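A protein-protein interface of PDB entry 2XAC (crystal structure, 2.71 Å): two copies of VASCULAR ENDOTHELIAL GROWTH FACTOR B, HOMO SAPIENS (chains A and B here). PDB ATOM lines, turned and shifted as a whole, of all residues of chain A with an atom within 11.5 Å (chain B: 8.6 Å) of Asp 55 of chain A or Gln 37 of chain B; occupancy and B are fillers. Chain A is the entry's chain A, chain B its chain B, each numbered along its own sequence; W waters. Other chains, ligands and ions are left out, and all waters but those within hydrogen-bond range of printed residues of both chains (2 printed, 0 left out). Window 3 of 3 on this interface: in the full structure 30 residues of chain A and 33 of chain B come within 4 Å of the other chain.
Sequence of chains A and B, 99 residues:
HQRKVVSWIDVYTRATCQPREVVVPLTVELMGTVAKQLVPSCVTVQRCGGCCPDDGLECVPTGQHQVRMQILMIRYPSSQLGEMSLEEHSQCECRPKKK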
ATOM      1  N   TRP A   8     -36.347  -2.556   0.432  1.00  0.00           N
ATOM      2  CA  TRP A   8     -35.221  -1.669   0.227  1.00  0.00           C
ATOM      3  C   TRP A   8     -34.125  -2.581  -0.252  1.00  0.00           C
ATOM      4  O   TRP A   8     -33.933  -3.673   0.282  1.00  0.00           O
ATOM      5  CB  TRP A   8     -34.818  -0.991   1.535  1.00  0.00           C
ATOM      6  CG  TRP A   8     -33.934   0.203   1.345  1.00  0.00           C
ATOM      7  CD1 TRP A   8     -34.241   1.504   1.620  1.00  0.00           C
ATOM      8  CD2 TRP A   8     -32.595   0.208   0.833  1.00  0.00           C
ATOM      9  NE1 TRP A   8     -33.177   2.317   1.313  1.00  0.00           N
ATOM     10  CE2 TRP A   8     -32.155   1.546   0.829  1.00  0.00           C
ATOM     11  CE3 TRP A   8     -31.726  -0.790   0.380  1.00  0.00           C
ATOM     12  CZ2 TRP A   8     -30.884   1.913   0.388  1.00  0.00           C
ATOM     13  CZ3 TRP A   8     -30.466  -0.425  -0.056  1.00  0.00           C
ATOM     14  CH2 TRP A   8     -30.057   0.915  -0.049  1.00  0.00           C
ATOM     15  N   TYR A  12     -34.096   0.351  -4.358  1.00  0.00           N
ATOM     16  CA  TYR A  12     -32.922   1.104  -4.805  1.00  0.00           C
ATOM     17  C   TYR A  12     -32.502   0.733  -6.226  1.00  0.00           C
ATOM     18  O   TYR A  12     -32.492   1.599  -7.100  1.00  0.00           O
ATOM     19  CB  TYR A  12     -31.743   0.967  -3.834  1.00  0.00           C
ATOM     20  CG  TYR A  12     -30.651   1.989  -4.092  1.00  0.00           C
ATOM     21  CD1 TYR A  12     -30.785   3.311  -3.656  1.00  0.00           C
ATOM     22  CD2 TYR A  12     -29.492   1.643  -4.786  1.00  0.00           C
ATOM     23  CE1 TYR A  12     -29.794   4.263  -3.901  1.00  0.00           C
ATOM     24  CE2 TYR A  12     -28.489   2.587  -5.034  1.00  0.00           C
ATOM     25  CZ  TYR A  12     -28.649   3.895  -4.590  1.00  0.00           C
ATOM     26  OH  TYR A  12     -27.661   4.826  -4.835  1.00  0.00           O
ATOM     27  N   GLY A  50     -33.862   7.249 -13.698  1.00  0.00           N
ATOM     28  CA  GLY A  50     -33.472   6.914 -12.340  1.00  0.00           C
ATOM     29  C   GLY A  50     -32.800   8.117 -11.711  1.00  0.00           C
ATOM     30  O   GLY A  50     -32.975   9.253 -12.174  1.00  0.00           O
ATOM     31  N   CYS A  51     -32.025   7.869 -10.659  1.00  0.00           N
ATOM     32  CA  CYS A  51     -31.327   8.940  -9.957  1.00  0.00           C
ATOM     33  C   CYS A  51     -30.000   8.471  -9.379  1.00  0.00           C
ATOM     34  O   CYS A  51     -29.792   7.274  -9.130  1.00  0.00           O
ATOM     35  CB  CYS A  51     -32.201   9.500  -8.841  1.00  0.00           C
ATOM     36  SG  CYS A  51     -32.684   8.248  -7.643  1.00  0.00           S
ATOM     37  N   CYS A  52     -29.110   9.438  -9.172  1.00  0.00           N
ATOM     38  CA  CYS A  52     -27.828   9.208  -8.532  1.00  0.00           C
ATOM     39  C   CYS A  52     -27.985   9.307  -7.020  1.00  0.00           C
ATOM     40  O   CYS A  52     -29.024   9.753  -6.542  1.00  0.00           O
ATOM     41  CB  CYS A  52     -26.818  10.229  -9.039  1.00  0.00           C
ATOM     42  SG  CYS A  52     -26.472  10.067 -10.792  1.00  0.00           S
ATOM     43  N   PRO A  53     -26.969   8.870  -6.255  1.00  0.00           N
ATOM     44  CA  PRO A  53     -27.127   8.970  -4.808  1.00  0.00           C
ATOM     45  C   PRO A  53     -26.775  10.362  -4.272  1.00  0.00           C
ATOM     46  O   PRO A  53     -26.625  10.534  -3.062  1.00  0.00           O
ATOM     47  CB  PRO A  53     -26.158   7.909  -4.280  1.00  0.00           C
ATOM     48  CG  PRO A  53     -25.095   7.835  -5.304  1.00  0.00           C
ATOM     49  CD  PRO A  53     -25.725   8.164  -6.628  1.00  0.00           C
ATOM     50  N   ASP A  54     -26.659  11.343  -5.164  1.00  0.00           N
ATOM     51  CA  ASP A  54     -26.359  12.712  -4.758  1.00  0.00           C
ATOM     52  C   ASP A  54     -27.012  13.769  -5.628  1.00  0.00           C
ATOM     53  O   ASP A  54     -27.356  13.505  -6.781  1.00  0.00           O
ATOM     54  CB  ASP A  54     -24.847  12.942  -4.718  1.00  0.00           C
ATOM     55  CG  ASP A  54     -24.294  12.937  -3.306  1.00  0.00           C
ATOM     56  OD1 ASP A  54     -25.061  13.256  -2.366  1.00  0.00           O
ATOM     57  OD2 ASP A  54     -23.094  12.623  -3.135  1.00  0.00           O
ATOM     58  N   ASP A  55     -27.180  14.961  -5.047  1.00  0.00           N
ATOM     59  CA  ASP A  55     -27.504  16.184  -5.785  1.00  0.00           C
ATOM     60  C   ASP A  55     -26.382  16.496  -6.765  1.00  0.00           C
ATOM     61  O   ASP A  55     -26.624  16.997  -7.865  1.00  0.00           O
ATOM     62  CB  ASP A  55     -27.640  17.368  -4.829  1.00  0.00           C
ATOM     63  CG  ASP A  55     -28.942  17.356  -4.056  1.00  0.00           C
ATOM     64  OD1 ASP A  55     -30.017  17.506  -4.680  1.00  0.00           O
ATOM     65  OD2 ASP A  55     -28.884  17.220  -2.814  1.00  0.00           O
ATOM     66  N   GLY A  56     -25.153  16.205  -6.338  1.00  0.00           N
ATOM     67  CA  GLY A  56     -23.955  16.443  -7.138  1.00  0.00           C
ATOM     68  C   GLY A  56     -23.871  15.586  -8.383  1.00  0.00           C
ATOM     69  O   GLY A  56     -23.591  16.092  -9.467  1.00  0.00           O
ATOM     70  N   LEU A  57     -24.117  14.288  -8.232  1.00  0.00           N
ATOM     71  CA  LEU A  57     -24.020  13.370  -9.361  1.00  0.00           C
ATOM     72  C   LEU A  57     -25.282  13.376 -10.222  1.00  0.00           C
ATOM     73  O   LEU A  57     -26.401  13.367  -9.706  1.00  0.00           O
ATOM     74  CB  LEU A  57     -23.713  11.949  -8.882  1.00  0.00           C
ATOM     75  CG  LEU A  57     -22.439  11.675  -8.082  1.00  0.00           C
ATOM     76  CD1 LEU A  57     -22.408  10.231  -7.643  1.00  0.00           C
ATOM     77  CD2 LEU A  57     -21.203  12.000  -8.887  1.00  0.00           C
ATOM     78  N   GLU A  58     -25.088  13.395 -11.538  1.00  0.00           N
ATOM     79  CA  GLU A  58     -26.198  13.313 -12.485  1.00  0.00           C
ATOM     80  C   GLU A  58     -26.090  12.094 -13.403  1.00  0.00           C
ATOM     81  O   GLU A  58     -25.006  11.751 -13.876  1.00  0.00           O
ATOM     82  CB  GLU A  58     -26.325  14.598 -13.305  1.00  0.00           C
ATOM     83  CG  GLU A  58     -25.159  14.896 -14.245  1.00  0.00           C
ATOM     84  CD  GLU A  58     -25.422  16.113 -15.119  1.00  0.00           C
ATOM     85  OE1 GLU A  58     -26.308  16.923 -14.756  1.00  0.00           O
ATOM     86  OE2 GLU A  58     -24.750  16.260 -16.167  1.00  0.00           O
ATOM     87  N   CYS A  59     -27.234  11.449 -13.631  1.00  0.00           N
ATOM     88  CA  CYS A  59     -27.328  10.264 -14.470  1.00  0.00           C
ATOM     89  C   CYS A  59     -27.209  10.639 -15.944  1.00  0.00           C
ATOM     90  O   CYS A  59     -28.140  11.201 -16.525  1.00  0.00           O
ATOM     91  CB  CYS A  59     -28.651   9.549 -14.205  1.00  0.00           C
ATOM     92  SG  CYS A  59     -28.851   7.972 -15.067  1.00  0.00           S
ATOM     93  N   VAL A  60     -26.052  10.334 -16.534  1.00  0.00           N
ATOM     94  CA  VAL A  60     -25.761  10.657 -17.937  1.00  0.00           C
ATOM     95  C   VAL A  60     -25.438   9.406 -18.769  1.00  0.00           C
ATOM     96  O   VAL A  60     -25.124   8.353 -18.206  1.00  0.00           O
ATOM     97  CB  VAL A  60     -24.614  11.691 -18.068  1.00  0.00           C
ATOM     98  CG1 VAL A  60     -25.087  13.081 -17.661  1.00  0.00           C
ATOM     99  CG2 VAL A  60     -23.410  11.271 -17.251  1.00  0.00           C
ATOM    100  N   CYS A  94     -23.779   7.422 -13.593  1.00  0.00           N
ATOM    101  CA  CYS A  94     -23.937   8.535 -12.669  1.00  0.00           C
ATOM    102  C   CYS A  94     -22.642   9.324 -12.571  1.00  0.00           C
ATOM    103  O   CYS A  94     -21.660   8.837 -12.008  1.00  0.00           O
ATOM    104  CB  CYS A  94     -24.348   8.022 -11.293  1.00  0.00           C
ATOM    105  SG  CYS A  94     -26.112   8.074 -11.019  1.00  0.00           S
ATOM    106  N   ARG A  95     -22.638  10.538 -13.117  1.00  0.00           N
ATOM    107  CA  ARG A  95     -21.424  11.363 -13.138  1.00  0.00           C
ATOM    108  C   ARG A  95     -21.589  12.732 -12.463  1.00  0.00           C
ATOM    109  O   ARG A  95     -22.710  13.223 -12.329  1.00  0.00           O
ATOM    110  CB  ARG A  95     -20.915  11.535 -14.572  1.00  0.00           C
ATOM    111  CG  ARG A  95     -20.532  10.226 -15.264  1.00  0.00           C
ATOM    112  CD  ARG A  95     -19.279  10.391 -16.116  1.00  0.00           C
ATOM    113  NE  ARG A  95     -19.466  11.304 -17.244  1.00  0.00           N
ATOM    114  CZ  ARG A  95     -18.475  11.796 -17.983  1.00  0.00           C
ATOM    115  NH1 ARG A  95     -17.214  11.480 -17.715  1.00  0.00           N
ATOM    116  NH2 ARG A  95     -18.743  12.614 -18.994  1.00  0.00           N
ATOM    117  N   PRO A  96     -20.466  13.344 -12.026  1.00  0.00           N
ATOM    118  CA  PRO A  96     -20.467  14.698 -11.454  1.00  0.00           C
ATOM    119  C   PRO A  96     -21.010  15.744 -12.420  1.00  0.00           C
ATOM    120  O   PRO A  96     -20.849  15.608 -13.636  1.00  0.00           O
ATOM    121  CB  PRO A  96     -18.983  14.971 -11.191  1.00  0.00           C
ATOM    122  CG  PRO A  96     -18.375  13.631 -11.026  1.00  0.00           C
ATOM    123  CD  PRO A  96     -19.130  12.721 -11.947  1.00  0.00           C
ATOM    124  N   LYS A  97     -21.629  16.787 -11.868  1.00  0.00           N
ATOM    125  CA  LYS A  97     -22.247  17.859 -12.659  1.00  0.00           C
ATOM    126  C   LYS A  97     -21.256  18.920 -13.187  1.00  0.00           C
ATOM    127  O   LYS A  97     -20.032  18.731 -13.146  1.00  0.00           O
ATOM    128  CB  LYS A  97     -23.383  18.512 -11.856  1.00  0.00           C
ATOM    129  CG  LYS A  97     -24.665  17.692 -11.834  1.00  0.00           C
ATOM    130  CD  LYS A  97     -25.745  18.320 -10.965  1.00  0.00           C
ATOM    131  CE  LYS A  97     -27.050  17.531 -11.063  1.00  0.00           C
ATOM    132  NZ  LYS A  97     -28.142  18.118 -10.240  1.00  0.00           N
ATOM    133  N   LYS A  98     -21.807  20.020 -13.702  1.00  0.00           N
ATOM    134  CA  LYS A  98     -21.032  21.166 -14.185  1.00  0.00           C
ATOM    135  C   LYS A  98     -21.473  22.429 -13.442  1.00  0.00           C
ATOM    136  O   LYS A  98     -22.561  22.462 -12.854  1.00  0.00           O
ATOM    137  CB  LYS A  98     -21.247  21.376 -15.690  1.00  0.00           C
ATOM    138  CG  LYS A  98     -21.657  20.131 -16.481  1.00  0.00           C
ATOM    139  CD  LYS A  98     -22.173  20.490 -17.874  1.00  0.00           C
ATOM    140  CE  LYS A  98     -23.461  21.315 -17.816  1.00  0.00           C
ATOM    141  NZ  LYS A  98     -23.921  21.725 -19.171  1.00  0.00           N
ATOM    142  N   LYS A  99     -20.638  23.469 -13.483  1.00  0.00           N
ATOM    143  CA  LYS A  99     -20.960  24.744 -12.831  1.00  0.00           C
ATOM    144  C   LYS A  99     -21.551  25.734 -13.835  1.00  0.00           C
ATOM    145  O   LYS A  99     -21.618  25.443 -15.030  1.00  0.00           O
ATOM    146  CB  LYS A  99     -19.718  25.335 -12.154  1.00  0.00           C
ATOM    147  CG  LYS A  99     -19.910  25.700 -10.676  1.00  0.00           C
ATOM    148  CD  LYS A  99     -20.907  26.850 -10.446  1.00  0.00           C
ATOM    149  CE  LYS A  99     -20.271  28.226 -10.661  1.00  0.00           C
ATOM    150  NZ  LYS A  99     -21.172  29.331 -10.227  1.00  0.00           N
ATOM    151  OXT LYS A  99     -21.984  26.840 -13.491  1.00  0.00           O
ATOM    152  N   LEU B  26     -38.710  11.899  -5.298  1.00  0.00           N
ATOM    153  CA  LEU B  26     -39.395  11.928  -4.003  1.00  0.00           C
ATOM    154  C   LEU B  26     -39.115  13.188  -3.178  1.00  0.00           C
ATOM    155  O   LEU B  26     -38.885  13.114  -1.962  1.00  0.00           O
ATOM    156  CB  LEU B  26     -39.063  10.663  -3.208  1.00  0.00           C
ATOM    157  CG  LEU B  26     -39.400   9.357  -3.924  1.00  0.00           C
ATOM    158  CD1 LEU B  26     -38.904   8.185  -3.115  1.00  0.00           C
ATOM    159  CD2 LEU B  26     -40.893   9.248  -4.189  1.00  0.00           C
ATOM    160  N   THR B  27     -39.155  14.340  -3.851  1.00  0.00           N
ATOM    161  CA  THR B  27     -38.962  15.642  -3.208  1.00  0.00           C
ATOM    162  C   THR B  27     -40.286  16.286  -2.801  1.00  0.00           C
ATOM    163  O   THR B  27     -40.365  16.960  -1.768  1.00  0.00           O
ATOM    164  CB  THR B  27     -38.180  16.621  -4.127  1.00  0.00           C
ATOM    165  OG1 THR B  27     -38.187  17.939  -3.552  1.00  0.00           O
ATOM    166  CG2 THR B  27     -38.792  16.667  -5.544  1.00  0.00           C
ATOM    167  N   MET B  31     -40.253  16.608   3.487  1.00  0.00           N
ATOM    168  CA  MET B  31     -38.815  16.390   3.539  1.00  0.00           C
ATOM    169  C   MET B  31     -38.119  17.161   4.662  1.00  0.00           C
ATOM    170  O   MET B  31     -37.346  18.095   4.420  1.00  0.00           O
ATOM    171  CB  MET B  31     -38.161  16.649   2.181  1.00  0.00           C
ATOM    172  CG  MET B  31     -37.188  15.556   1.783  1.00  0.00           C
ATOM    173  SD  MET B  31     -35.744  16.193   0.915  1.00  0.00           S
ATOM    174  CE  MET B  31     -34.745  16.767   2.298  1.00  0.00           C
ATOM    175  N   GLY B  32     -38.399  16.761   5.898  1.00  0.00           N
ATOM    176  CA  GLY B  32     -37.809  17.400   7.059  1.00  0.00           C
ATOM    177  C   GLY B  32     -37.354  16.397   8.101  1.00  0.00           C
ATOM    178  O   GLY B  32     -36.325  16.584   8.749  1.00  0.00           O
ATOM    179  N   THR B  33     -38.127  15.327   8.261  1.00  0.00           N
ATOM    180  CA  THR B  33     -37.805  14.291   9.225  1.00  0.00           C
ATOM    181  C   THR B  33     -36.824  14.762  10.280  1.00  0.00           C
ATOM    182  O   THR B  33     -36.966  15.852  10.833  1.00  0.00           O
ATOM    183  N   VAL B  34     -35.822  13.933  10.561  1.00  0.00           N
ATOM    184  CA  VAL B  34     -34.756  14.248  11.550  1.00  0.00           C
ATOM    185  C   VAL B  34     -33.567  14.961  10.915  1.00  0.00           C
ATOM    186  O   VAL B  34     -32.498  15.062  11.515  1.00  0.00           O
ATOM    187  CB  VAL B  34     -34.308  13.007  12.291  1.00  0.00           C
ATOM    188  CG1 VAL B  34     -35.424  12.404  13.132  1.00  0.00           C
ATOM    189  CG2 VAL B  34     -33.772  11.990  11.295  1.00  0.00           C
ATOM    190  N   ALA B  35     -33.763  15.455   9.696  1.00  0.00           N
ATOM    191  CA  ALA B  35     -32.713  16.155   8.980  1.00  0.00           C
ATOM    192  C   ALA B  35     -31.878  15.231   8.194  1.00  0.00           C
ATOM    193  O   ALA B  35     -31.151  14.419   8.765  1.00  0.00           O
ATOM    194  N   LYS B  36     -31.938  15.343   6.870  1.00  0.00           N
ATOM    195  CA  LYS B  36     -31.137  14.503   5.998  1.00  0.00           C
ATOM    196  C   LYS B  36     -31.793  14.281   4.649  1.00  0.00           C
ATOM    197  O   LYS B  36     -32.514  15.143   4.147  1.00  0.00           O
ATOM    198  N   GLN B  37     -31.541  13.116   4.060  1.00  0.00           N
ATOM    199  CA  GLN B  37     -32.111  12.775   2.756  1.00  0.00           C
ATOM    200  C   GLN B  37     -32.591  11.331   2.683  1.00  0.00           C
ATOM    201  O   GLN B  37     -32.041  10.443   3.338  1.00  0.00           O
ATOM    202  CB  GLN B  37     -31.121  13.069   1.626  1.00  0.00           C
ATOM    203  CG  GLN B  37     -31.035  14.547   1.262  1.00  0.00           C
ATOM    204  CD  GLN B  37     -30.612  14.789  -0.179  1.00  0.00           C
ATOM    205  OE1 GLN B  37     -30.232  13.861  -0.901  1.00  0.00           O
ATOM    206  NE2 GLN B  37     -30.682  16.045  -0.606  1.00  0.00           N
ATOM    207  N   LEU B  38     -33.631  11.116   1.884  1.00  0.00           N
ATOM    208  CA  LEU B  38     -34.180   9.787   1.657  1.00  0.00           C
ATOM    209  C   LEU B  38     -33.295   9.047   0.667  1.00  0.00           C
ATOM    210  O   LEU B  38     -32.680   9.667  -0.203  1.00  0.00           O
ATOM    211  CB  LEU B  38     -35.619   9.876   1.127  1.00  0.00           C
ATOM    212  CG  LEU B  38     -36.774  10.227   2.081  1.00  0.00           C
ATOM    213  CD1 LEU B  38     -36.892  11.733   2.320  1.00  0.00           C
ATOM    214  CD2 LEU B  38     -38.089   9.682   1.542  1.00  0.00           C
ATOM    215  N   VAL B  39     -33.219   7.726   0.816  1.00  0.00           N
ATOM    216  CA  VAL B  39     -32.416   6.886  -0.073  1.00  0.00           C
ATOM    217  C   VAL B  39     -33.185   5.620  -0.467  1.00  0.00           C
ATOM    218  O   VAL B  39     -33.560   4.831   0.397  1.00  0.00           O
ATOM    219  CB  VAL B  39     -31.037   6.519   0.541  1.00  0.00           C
ATOM    220  CG1 VAL B  39     -30.186   5.762  -0.469  1.00  0.00           C
ATOM    221  CG2 VAL B  39     -30.297   7.765   0.998  1.00  0.00           C
ATOM    222  N   PRO B  40     -33.434   5.432  -1.778  1.00  0.00           N
ATOM    223  CA  PRO B  40     -33.065   6.360  -2.852  1.00  0.00           C
ATOM    224  C   PRO B  40     -33.888   7.648  -2.825  1.00  0.00           C
ATOM    225  O   PRO B  40     -34.937   7.700  -2.184  1.00  0.00           O
ATOM    226  CB  PRO B  40     -33.371   5.565  -4.127  1.00  0.00           C
ATOM    227  CG  PRO B  40     -34.383   4.566  -3.721  1.00  0.00           C
ATOM    228  CD  PRO B  40     -34.053   4.204  -2.308  1.00  0.00           C
ATOM    229  N   SER B  41     -33.399   8.672  -3.518  1.00  0.00           N
ATOM    230  CA  SER B  41     -34.098   9.950  -3.622  1.00  0.00           C
ATOM    231  C   SER B  41     -35.031   9.999  -4.844  1.00  0.00           C
ATOM    232  O   SER B  41     -35.382  11.075  -5.340  1.00  0.00           O
ATOM    233  CB  SER B  41     -33.088  11.109  -3.628  1.00  0.00           C
ATOM    234  OG  SER B  41     -31.988  10.859  -4.494  1.00  0.00           O
ATOM    235  N   CYS B  42     -35.431   8.817  -5.311  1.00  0.00           N
ATOM    236  CA  CYS B  42     -36.328   8.656  -6.458  1.00  0.00           C
ATOM    237  C   CYS B  42     -36.815   7.214  -6.517  1.00  0.00           C
ATOM    238  O   CYS B  42     -36.136   6.312  -6.021  1.00  0.00           O
ATOM    239  CB  CYS B  42     -35.603   8.974  -7.763  1.00  0.00           C
ATOM    240  SG  CYS B  42     -34.509   7.653  -8.308  1.00  0.00           S
ATOM    241  N   ILE B  71     -38.041   2.843   2.371  1.00  0.00           N
ATOM    242  CA  ILE B  71     -37.072   3.894   2.082  1.00  0.00           C
ATOM    243  C   ILE B  71     -36.248   4.232   3.314  1.00  0.00           C
ATOM    244  O   ILE B  71     -36.781   4.408   4.413  1.00  0.00           O
ATOM    245  CB  ILE B  71     -37.735   5.165   1.514  1.00  0.00           C
ATOM    246  CG1 ILE B  71     -38.405   4.848   0.181  1.00  0.00           C
ATOM    247  CG2 ILE B  71     -36.698   6.262   1.304  1.00  0.00           C
ATOM    248  CD1 ILE B  71     -39.218   5.974  -0.383  1.00  0.00           C
ATOM    249  N   LEU B  72     -34.940   4.315   3.096  1.00  0.00           N
ATOM    250  CA  LEU B  72     -33.969   4.620   4.124  1.00  0.00           C
ATOM    251  C   LEU B  72     -33.738   6.126   4.163  1.00  0.00           C
ATOM    252  O   LEU B  72     -33.481   6.745   3.131  1.00  0.00           O
ATOM    253  CB  LEU B  72     -32.673   3.885   3.789  1.00  0.00           C
ATOM    254  CG  LEU B  72     -31.508   3.771   4.766  1.00  0.00           C
ATOM    255  CD1 LEU B  72     -31.927   3.143   6.090  1.00  0.00           C
ATOM    256  CD2 LEU B  72     -30.449   2.923   4.095  1.00  0.00           C
ATOM    257  N   MET B  73     -33.846   6.713   5.352  1.00  0.00           N
ATOM    258  CA  MET B  73     -33.633   8.152   5.520  1.00  0.00           C
ATOM    259  C   MET B  73     -32.380   8.402   6.346  1.00  0.00           C
ATOM    260  O   MET B  73     -32.418   8.320   7.577  1.00  0.00           O
ATOM    261  CB  MET B  73     -34.843   8.821   6.186  1.00  0.00           C
ATOM    262  CG  MET B  73     -36.186   8.598   5.486  1.00  0.00           C
ATOM    263  SD  MET B  73     -37.133   7.198   6.131  1.00  0.00           S
ATOM    264  CE  MET B  73     -37.655   7.833   7.729  1.00  0.00           C
ATOM    265  N   ILE B  74     -31.270   8.697   5.670  1.00  0.00           N
ATOM    266  CA  ILE B  74     -29.994   8.945   6.350  1.00  0.00           C
ATOM    267  C   ILE B  74     -30.036  10.250   7.144  1.00  0.00           C
ATOM    268  O   ILE B  74     -30.568  11.261   6.671  1.00  0.00           O
ATOM    269  CB  ILE B  74     -28.764   8.919   5.382  1.00  0.00           C
ATOM    270  CG1 ILE B  74     -28.793  10.098   4.395  1.00  0.00           C
ATOM    271  CG2 ILE B  74     -28.677   7.573   4.647  1.00  0.00           C
ATOM    272  CD1 ILE B  74     -27.422  10.503   3.851  1.00  0.00           C
ATOM    273  N   ARG B  75     -29.476  10.224   8.349  1.00  0.00           N
ATOM    274  CA  ARG B  75     -29.449  11.396   9.203  1.00  0.00           C
ATOM    275  C   ARG B  75     -28.909  11.093  10.587  1.00  0.00           C
ATOM    276  O   ARG B  75     -28.024  10.253  10.750  1.00  0.00           O
ATOM    277  N   TYR B  76     -29.446  11.782  11.590  1.00  0.00           N
ATOM    278  CA  TYR B  76     -29.017  11.587  12.968  1.00  0.00           C
ATOM    279  C   TYR B  76     -29.998  10.704  13.733  1.00  0.00           C
ATOM    280  O   TYR B  76     -31.165  11.058  13.902  1.00  0.00           O
ATOM    281  CB  TYR B  76     -28.862  12.935  13.677  1.00  0.00           C
ATOM    282  CG  TYR B  76     -28.769  12.829  15.182  1.00  0.00           C
ATOM    283  CD1 TYR B  76     -28.614  13.963  15.969  1.00  0.00           C
ATOM    284  CD2 TYR B  76     -28.835  11.596  15.817  1.00  0.00           C
ATOM    285  CE1 TYR B  76     -28.528  13.872  17.345  1.00  0.00           C
ATOM    286  CE2 TYR B  76     -28.751  11.495  17.192  1.00  0.00           C
ATOM    287  CZ  TYR B  76     -28.597  12.635  17.951  1.00  0.00           C
ATOM    288  OH  TYR B  76     -28.512  12.539  19.321  1.00  0.00           O
ATOM    289  N   SER B  79     -29.225   6.246  11.613  1.00  0.00           N
ATOM    290  CA  SER B  79     -30.539   6.553  11.059  1.00  0.00           C
ATOM    291  C   SER B  79     -31.426   5.383  10.614  1.00  0.00           C
ATOM    292  O   SER B  79     -30.948   4.352  10.264  1.00  0.00           O
ATOM    293  CB  SER B  79     -30.289   7.446   9.888  1.00  0.00           C
ATOM    294  OG  SER B  79     -28.934   7.350   9.536  1.00  0.00           O
ATOM    295  N   GLN B  80     -32.725   5.581  10.587  1.00  0.00           N
ATOM    296  CA  GLN B  80     -33.657   4.496  10.482  1.00  0.00           C
ATOM    297  C   GLN B  80     -34.419   4.383   9.198  1.00  0.00           C
ATOM    298  O   GLN B  80     -34.617   5.327   8.502  1.00  0.00           O
ATOM    299  CB  GLN B  80     -34.616   4.570  11.608  1.00  0.00           C
HETATM  300  O   HOH W   1     -30.611   7.855  -4.567  1.00  0.00           O
HETATM  301  O   HOH W   2     -29.900  10.725  -2.547  1.00  0.00           O
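NE2 of Gln 37 of chain B sits at hydrogen-bond distance from OD2 of Asp 55 of chain A (3.1 Å).
The indole nitrogen (NE1) of Trp 8 of chain A sits close to the backbone NH (N) of Leu 72 of chain B, 3.2 Å away.
SG of Cys 51 of chain A forms a disulfide with SG of Cys 42 of chain B, 2.0 Å away.
NE1 of Trp 8 of chain A lies within hydrogen-bond range of O of Val 39 of chain B (2.7 Å).
The backbone NH of Cys 59 of chain A sits at hydrogen-bond distance from the side-chain sulfur of Cys 52 of chain A, at 3.2 Å.
The backbone NH (N) of Val 39 of chain B sits at hydrogen-bond distance from the backbone carbonyl oxygen (O) of Leu 72 of chain B (2.5 Å).
The side-chain sulfur of Cys 52 of chain A lies close to the backbone NH of Glu 58 of chain A, at 3.7 Å.
N of Ile 74 of chain B sits at hydrogen-bond distance from O of Gln 37 of chain B, 3.0 Å away.
N of Leu 26 of chain B sits at hydrogen-bond distance from O of Ser 41 of chain B (3.4 Å).
SG of Cys 52 of chain A forms a disulfide with SG of Cys 94 of chain A (2.0 Å).
Among the printed residues, pairs that only touch across the chains: Tyr 12 of chain A with Pro 40 of chain B, Trp 8 of chain A with Ile 71 of chain B, Tyr 12 of chain A with Val 39 of chain B, Cys 52 of chain A with Ser 41 of chain B and Gly 50 of chain A with Cys 42 of chain B.
Of chain B, only Gln 37 (3.1 Å) comes within 4 Å of Asp 55 of chain A.
Of chain A, only Asp 55 comes within 4 Å of Gln 37 of chain B.
No residue of chain A comes within 4 Å of Ala 35 of chain B.
No residue of chain A comes within 4 Å of Lys 36 of chain B.
Leu 38 of chain B touches none of the printed residues of chain A.
Of chain A, only Trp 8 and Tyr 12 come within 4 Å of Val 39 of chain B.
Ser 41 of chain B touches just one residue of chain A: Cys 52 (3.8 Å).
Of the printed residues of chain A, Leu 72 of chain B touches Trp 8.
Printed residues of chain A within 4 Å of Pro 40 of chain B: Tyr 12.
Printed residues of chain A within 4 Å of Cys 42 of chain B: Gly 50 and Cys 51.
Of the printed residues of chain B, Gly 50 of chain A touches Cys 42 (3.8 Å).
Printed residues of chain B within 4 Å of Cys 52 of chain A: Ser 41.
The nearest residue of chain A that does not touch Gln 37 of chain B is Pro 53 of chain A (5.4 Å).
Of the 22 printed residues of chain B, 7 touch a printed residue of chain A.
Of the 19 printed residues of chain A, 6 touch a printed residue of chain B.
Printed residues of chain A that touch a printed residue of chain B: Trp 8, Tyr 12, Gly 50, Cys 51, Cys 52 and Asp 55.
Hydrophobic or aromatic side chains of chain A that line the printed part of chain B: Trp 8 and Tyr 12.
Among the printed residues, no Asp or Glu carboxylate lies within 4 Å of a Lys or Arg side-chain nitrogen of the other chain.
No position is printed for both chains.
Water W2 lies within hydrogen-bond range of the side-chain hydroxyl of Ser 41 of chain B (2.9 Å) and the backbone carbonyl oxygen of Pro 53 of chain A (3.3 Å).
Water W1 lies within hydrogen-bond range of N of Ser 41 of chain B, O of Cys 52 of chain A and SG of Cys 51 of chain A.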
